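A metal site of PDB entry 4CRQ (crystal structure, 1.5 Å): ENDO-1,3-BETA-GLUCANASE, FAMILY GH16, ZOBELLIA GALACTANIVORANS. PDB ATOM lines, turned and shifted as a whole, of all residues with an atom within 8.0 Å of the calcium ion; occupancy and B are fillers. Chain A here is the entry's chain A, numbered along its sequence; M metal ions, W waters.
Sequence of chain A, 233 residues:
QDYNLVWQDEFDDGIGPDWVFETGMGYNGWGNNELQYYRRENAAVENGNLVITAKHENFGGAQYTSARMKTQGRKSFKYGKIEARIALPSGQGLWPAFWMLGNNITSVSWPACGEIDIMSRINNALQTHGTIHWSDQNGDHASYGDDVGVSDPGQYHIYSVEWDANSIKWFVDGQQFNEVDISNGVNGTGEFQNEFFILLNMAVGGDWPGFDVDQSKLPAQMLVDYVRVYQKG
Within 4 Å of the calcium ion: Glu 10, Gly 48 and Asp 225. The nearest printed residue that does not touch the calcium ion is Phe 11 (4.5 Å).
The side-chain carboxylate (OD2) of Asp 225 is in salt-bridge range of the guanidinium group (NH1) of Arg 85 (2.8 Å). The side-chain carboxylate of Glu 10 is in salt-bridge range of the guanidinium group of Arg 228, 2.8 Å away. N of Asp 225 sits close to OD1 of Asn 49.
O of Gly 48 is bound to the calcium ion (2.3 Å). O of Glu 10 binds the calcium ion (2.3 Å). Water W3 binds the calcium ion (2.3 Å). The calcium ion is bound by OD1 of Asp 225 (2.4 Å). The backbone carbonyl oxygen (O) of Asp 225 binds the calcium ion, at 2.4 Å. The calcium ion is bound by water W2 (2.5 Å). The calcium ion is bound by water W1.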
ATOM      1  N   ASP A   9     -22.877 -13.309   1.062  1.00  0.00           N
ATOM      2  CA  ASP A   9     -22.934 -13.596  -0.361  1.00  0.00           C
ATOM      3  C   ASP A   9     -21.709 -14.475  -0.586  1.00  0.00           C
ATOM      4  O   ASP A   9     -20.579 -13.992  -0.457  1.00  0.00           O
ATOM      5  CB  ASP A   9     -22.922 -12.370  -1.294  1.00  0.00           C
ATOM      6  CG  ASP A   9     -23.361 -12.741  -2.722  1.00  0.00           C
ATOM      7  OD1 ASP A   9     -23.222 -13.947  -3.103  1.00  0.00           O
ATOM      8  OD2 ASP A   9     -23.845 -11.872  -3.446  1.00  0.00           O
ATOM      9  N   GLU A  10     -21.927 -15.753  -0.912  1.00  0.00           N
ATOM     10  CA  GLU A  10     -20.858 -16.745  -1.138  1.00  0.00           C
ATOM     11  C   GLU A  10     -20.433 -16.817  -2.619  1.00  0.00           C
ATOM     12  O   GLU A  10     -19.470 -17.509  -2.935  1.00  0.00           O
ATOM     13  CB  GLU A  10     -21.317 -18.145  -0.698  1.00  0.00           C
ATOM     14  CG  GLU A  10     -21.692 -18.223   0.778  1.00  0.00           C
ATOM     15  CD  GLU A  10     -20.542 -17.917   1.731  1.00  0.00           C
ATOM     16  OE1 GLU A  10     -19.423 -18.434   1.506  1.00  0.00           O
ATOM     17  OE2 GLU A  10     -20.756 -17.160   2.713  1.00  0.00           O
ATOM     18  N   PHE A  11     -21.165 -16.124  -3.515  1.00  0.00           N
ATOM     19  CA  PHE A  11     -20.853 -16.142  -4.953  1.00  0.00           C
ATOM     20  C   PHE A  11     -20.732 -17.569  -5.530  1.00  0.00           C
ATOM     21  O   PHE A  11     -19.845 -17.826  -6.350  1.00  0.00           O
ATOM     22  CB  PHE A  11     -19.593 -15.269  -5.233  1.00  0.00           C
ATOM     23  CG  PHE A  11     -19.729 -13.848  -4.743  1.00  0.00           C
ATOM     24  CD1 PHE A  11     -20.641 -12.983  -5.358  1.00  0.00           C
ATOM     25  CD2 PHE A  11     -18.971 -13.399  -3.659  1.00  0.00           C
ATOM     26  CE1 PHE A  11     -20.781 -11.669  -4.894  1.00  0.00           C
ATOM     27  CE2 PHE A  11     -19.090 -12.064  -3.193  1.00  0.00           C
ATOM     28  CZ  PHE A  11     -20.014 -11.214  -3.823  1.00  0.00           C
ATOM     29  N   ASP A  12     -21.612 -18.498  -5.100  1.00  0.00           N
ATOM     30  CA  ASP A  12     -21.492 -19.892  -5.564  1.00  0.00           C
ATOM     31  C   ASP A  12     -21.488 -20.033  -7.083  1.00  0.00           C
ATOM     32  O   ASP A  12     -20.575 -20.638  -7.656  1.00  0.00           O
ATOM     33  CB  ASP A  12     -22.567 -20.797  -4.949  1.00  0.00           C
ATOM     34  CG  ASP A  12     -22.419 -20.979  -3.455  1.00  0.00           C
ATOM     35  OD1 ASP A  12     -21.336 -20.816  -2.868  1.00  0.00           O
ATOM     36  OD2 ASP A  12     -23.451 -21.315  -2.829  1.00  0.00           O
ATOM     37  N   ASP A  13     -22.503 -19.461  -7.723  1.00  0.00           N
ATOM     38  CA  ASP A  13     -22.697 -19.578  -9.187  1.00  0.00           C
ATOM     39  C   ASP A  13     -23.040 -18.270  -9.878  1.00  0.00           C
ATOM     40  O   ASP A  13     -22.916 -18.157 -11.119  1.00  0.00           O
ATOM     41  CB  ASP A  13     -23.774 -20.628  -9.480  1.00  0.00           C
ATOM     42  CG  ASP A  13     -23.341 -22.054  -9.133  1.00  0.00           C
ATOM     43  OD1 ASP A  13     -22.374 -22.565  -9.766  1.00  0.00           O
ATOM     44  OD2 ASP A  13     -23.965 -22.671  -8.240  1.00  0.00           O
ATOM     45  N   VAL A  45     -18.903 -14.062 -11.969  1.00  0.00           N
ATOM     46  CA  VAL A  45     -18.558 -15.083 -10.994  1.00  0.00           C
ATOM     47  C   VAL A  45     -17.849 -16.207 -11.733  1.00  0.00           C
ATOM     48  O   VAL A  45     -18.306 -16.619 -12.813  1.00  0.00           O
ATOM     49  CB  VAL A  45     -19.793 -15.584 -10.194  1.00  0.00           C
ATOM     50  CG1 VAL A  45     -19.582 -16.918  -9.475  1.00  0.00           C
ATOM     51  CG2 VAL A  45     -20.185 -14.521  -9.183  1.00  0.00           C
ATOM     52  N   GLU A  46     -16.749 -16.674 -11.150  1.00  0.00           N
ATOM     53  CA  GLU A  46     -15.984 -17.804 -11.676  1.00  0.00           C
ATOM     54  C   GLU A  46     -15.521 -18.633 -10.500  1.00  0.00           C
ATOM     55  O   GLU A  46     -14.939 -18.079  -9.566  1.00  0.00           O
ATOM     56  CB  GLU A  46     -14.732 -17.363 -12.458  1.00  0.00           C
ATOM     57  CG  GLU A  46     -14.947 -16.575 -13.741  1.00  0.00           C
ATOM     58  CD  GLU A  46     -13.632 -16.303 -14.469  1.00  0.00           C
ATOM     59  OE1 GLU A  46     -13.022 -17.259 -15.010  1.00  0.00           O
ATOM     60  OE2 GLU A  46     -13.189 -15.135 -14.527  1.00  0.00           O
ATOM     61  N   ASN A  47     -15.777 -19.952 -10.560  1.00  0.00           N
ATOM     62  CA  ASN A  47     -15.284 -20.900  -9.527  1.00  0.00           C
ATOM     63  C   ASN A  47     -15.546 -20.447  -8.087  1.00  0.00           C
ATOM     64  O   ASN A  47     -14.640 -20.471  -7.238  1.00  0.00           O
ATOM     65  CB  ASN A  47     -13.774 -21.184  -9.749  1.00  0.00           C
ATOM     66  CG  ASN A  47     -13.471 -21.711 -11.140  1.00  0.00           C
ATOM     67  OD1 ASN A  47     -14.170 -22.582 -11.666  1.00  0.00           O
ATOM     68  ND2 ASN A  47     -12.433 -21.168 -11.756  1.00  0.00           N
ATOM     69  N   GLY A  48     -16.783 -20.030  -7.823  1.00  0.00           N
ATOM     70  CA  GLY A  48     -17.176 -19.607  -6.476  1.00  0.00           C
ATOM     71  C   GLY A  48     -16.656 -18.264  -6.010  1.00  0.00           C
ATOM     72  O   GLY A  48     -16.730 -17.967  -4.809  1.00  0.00           O
ATOM     73  N   ASN A  49     -16.130 -17.447  -6.919  1.00  0.00           N
ATOM     74  CA  ASN A  49     -15.647 -16.143  -6.549  1.00  0.00           C
ATOM     75  C   ASN A  49     -16.343 -15.078  -7.386  1.00  0.00           C
ATOM     76  O   ASN A  49     -16.569 -15.284  -8.602  1.00  0.00           O
ATOM     77  CB  ASN A  49     -14.144 -15.970  -6.869  1.00  0.00           C
ATOM     78  CG  ASN A  49     -13.235 -16.758  -5.957  1.00  0.00           C
ATOM     79  OD1 ASN A  49     -12.702 -16.211  -5.015  1.00  0.00           O
ATOM     80  ND2 ASN A  49     -13.075 -18.037  -6.227  1.00  0.00           N
ATOM     81  N   LEU A  50     -16.631 -13.944  -6.750  1.00  0.00           N
ATOM     82  CA  LEU A  50     -16.851 -12.712  -7.503  1.00  0.00           C
ATOM     83  C   LEU A  50     -15.501 -12.314  -8.131  1.00  0.00           C
ATOM     84  O   LEU A  50     -14.463 -12.313  -7.452  1.00  0.00           O
ATOM     85  CB  LEU A  50     -17.341 -11.582  -6.604  1.00  0.00           C
ATOM     86  CG  LEU A  50     -17.383 -10.149  -7.157  1.00  0.00           C
ATOM     87  CD1 LEU A  50     -18.433 -10.071  -8.259  1.00  0.00           C
ATOM     88  CD2 LEU A  50     -17.619  -9.138  -6.042  1.00  0.00           C
ATOM     89  N   ARG A  85     -13.234 -12.478   2.120  1.00  0.00           N
ATOM     90  CA  ARG A  85     -12.037 -13.295   1.833  1.00  0.00           C
ATOM     91  C   ARG A  85     -11.657 -12.898   0.400  1.00  0.00           C
ATOM     92  O   ARG A  85     -12.383 -13.177  -0.543  1.00  0.00           O
ATOM     93  CB  ARG A  85     -12.354 -14.788   2.021  1.00  0.00           C
ATOM     94  CG  ARG A  85     -11.163 -15.695   1.693  1.00  0.00           C
ATOM     95  CD  ARG A  85     -11.388 -17.125   2.209  1.00  0.00           C
ATOM     96  NE  ARG A  85     -10.163 -17.909   2.031  1.00  0.00           N
ATOM     97  CZ  ARG A  85      -9.838 -18.555   0.917  1.00  0.00           C
ATOM     98  NH1 ARG A  85     -10.669 -18.574  -0.144  1.00  0.00           N
ATOM     99  NH2 ARG A  85      -8.684 -19.234   0.856  1.00  0.00           N
ATOM    100  N   TYR A 156      -5.219 -15.367  -0.960  1.00  0.00           N
ATOM    101  CA  TYR A 156      -6.395 -14.970  -0.183  1.00  0.00           C
ATOM    102  C   TYR A 156      -5.989 -14.523   1.232  1.00  0.00           C
ATOM    103  O   TYR A 156      -5.091 -15.103   1.852  1.00  0.00           O
ATOM    104  CB  TYR A 156      -7.439 -16.079  -0.052  1.00  0.00           C
ATOM    105  CG  TYR A 156      -8.176 -16.287  -1.346  1.00  0.00           C
ATOM    106  CD1 TYR A 156      -9.280 -15.465  -1.690  1.00  0.00           C
ATOM    107  CD2 TYR A 156      -7.785 -17.304  -2.237  1.00  0.00           C
ATOM    108  CE1 TYR A 156      -9.961 -15.654  -2.886  1.00  0.00           C
ATOM    109  CE2 TYR A 156      -8.445 -17.514  -3.431  1.00  0.00           C
ATOM    110  CZ  TYR A 156      -9.546 -16.697  -3.767  1.00  0.00           C
ATOM    111  OH  TYR A 156     -10.177 -16.978  -4.969  1.00  0.00           O
ATOM    112  N   VAL A 224     -13.101 -12.134  -4.927  1.00  0.00           N
ATOM    113  CA  VAL A 224     -13.800 -12.096  -3.632  1.00  0.00           C
ATOM    114  C   VAL A 224     -14.553 -13.443  -3.469  1.00  0.00           C
ATOM    115  O   VAL A 224     -15.561 -13.715  -4.166  1.00  0.00           O
ATOM    116  CB  VAL A 224     -14.764 -10.886  -3.508  1.00  0.00           C
ATOM    117  CG1 VAL A 224     -15.392 -10.831  -2.085  1.00  0.00           C
ATOM    118  CG2 VAL A 224     -14.074  -9.574  -3.841  1.00  0.00           C
ATOM    119  N   ASP A 225     -14.050 -14.277  -2.552  1.00  0.00           N
ATOM    120  CA  ASP A 225     -14.653 -15.586  -2.302  1.00  0.00           C
ATOM    121  C   ASP A 225     -16.024 -15.395  -1.642  1.00  0.00           C
ATOM    122  O   ASP A 225     -16.986 -16.101  -1.988  1.00  0.00           O
ATOM    123  CB  ASP A 225     -13.677 -16.394  -1.439  1.00  0.00           C
ATOM    124  CG  ASP A 225     -14.129 -17.842  -1.190  1.00  0.00           C
ATOM    125  OD1 ASP A 225     -15.127 -18.343  -1.816  1.00  0.00           O
ATOM    126  OD2 ASP A 225     -13.462 -18.507  -0.344  1.00  0.00           O
ATOM    127  N   TYR A 226     -16.137 -14.465  -0.696  1.00  0.00           N
ATOM    128  CA  TYR A 226     -17.427 -14.227  -0.049  1.00  0.00           C
ATOM    129  C   TYR A 226     -17.381 -12.942   0.700  1.00  0.00           C
ATOM    130  O   TYR A 226     -16.263 -12.446   0.997  1.00  0.00           O
ATOM    131  CB  TYR A 226     -17.803 -15.374   0.935  1.00  0.00           C
ATOM    132  CG  TYR A 226     -16.758 -15.700   1.999  1.00  0.00           C
ATOM    133  CD1 TYR A 226     -16.516 -14.830   3.108  1.00  0.00           C
ATOM    134  CD2 TYR A 226     -16.024 -16.909   1.934  1.00  0.00           C
ATOM    135  CE1 TYR A 226     -15.580 -15.153   4.103  1.00  0.00           C
ATOM    136  CE2 TYR A 226     -15.076 -17.230   2.923  1.00  0.00           C
ATOM    137  CZ  TYR A 226     -14.861 -16.360   4.007  1.00  0.00           C
ATOM    138  OH  TYR A 226     -13.956 -16.665   4.992  1.00  0.00           O
ATOM    139  N   VAL A 227     -18.538 -12.381   1.012  1.00  0.00           N
ATOM    140  CA  VAL A 227     -18.656 -11.292   1.996  1.00  0.00           C
ATOM    141  C   VAL A 227     -19.604 -11.853   3.071  1.00  0.00           C
ATOM    142  O   VAL A 227     -20.639 -12.443   2.721  1.00  0.00           O
ATOM    143  CB  VAL A 227     -19.256  -9.991   1.412  1.00  0.00           C
ATOM    144  CG1 VAL A 227     -19.396  -8.918   2.515  1.00  0.00           C
ATOM    145  CG2 VAL A 227     -18.426  -9.471   0.218  1.00  0.00           C
ATOM    146  N   ARG A 228     -19.253 -11.695   4.359  1.00  0.00           N
ATOM    147  CA  ARG A 228     -20.101 -12.187   5.451  1.00  0.00           C
ATOM    148  C   ARG A 228     -20.227 -11.126   6.513  1.00  0.00           C
ATOM    149  O   ARG A 228     -19.258 -10.363   6.788  1.00  0.00           O
ATOM    150  CB  ARG A 228     -19.540 -13.481   6.073  1.00  0.00           C
ATOM    151  CG  ARG A 228     -19.561 -14.677   5.147  1.00  0.00           C
ATOM    152  CD  ARG A 228     -18.815 -15.856   5.730  1.00  0.00           C
ATOM    153  NE  ARG A 228     -18.771 -16.972   4.781  1.00  0.00           N
ATOM    154  CZ  ARG A 228     -18.014 -18.064   4.893  1.00  0.00           C
ATOM    155  NH1 ARG A 228     -17.199 -18.240   5.943  1.00  0.00           N
ATOM    156  NH2 ARG A 228     -18.100 -18.990   3.939  1.00  0.00           N
HETATM  157 CA    CA M   1     -17.330 -18.403  -2.673  1.00  0.00          CA
HETATM  158  O   HOH W   1     -18.918 -20.292  -3.444  1.00  0.00           O
HETATM  159  O   HOH W   2     -16.308 -20.691  -3.042  1.00  0.00           O
HETATM  160  O   HOH W   3     -17.732 -19.074  -0.466  1.00  0.00           O
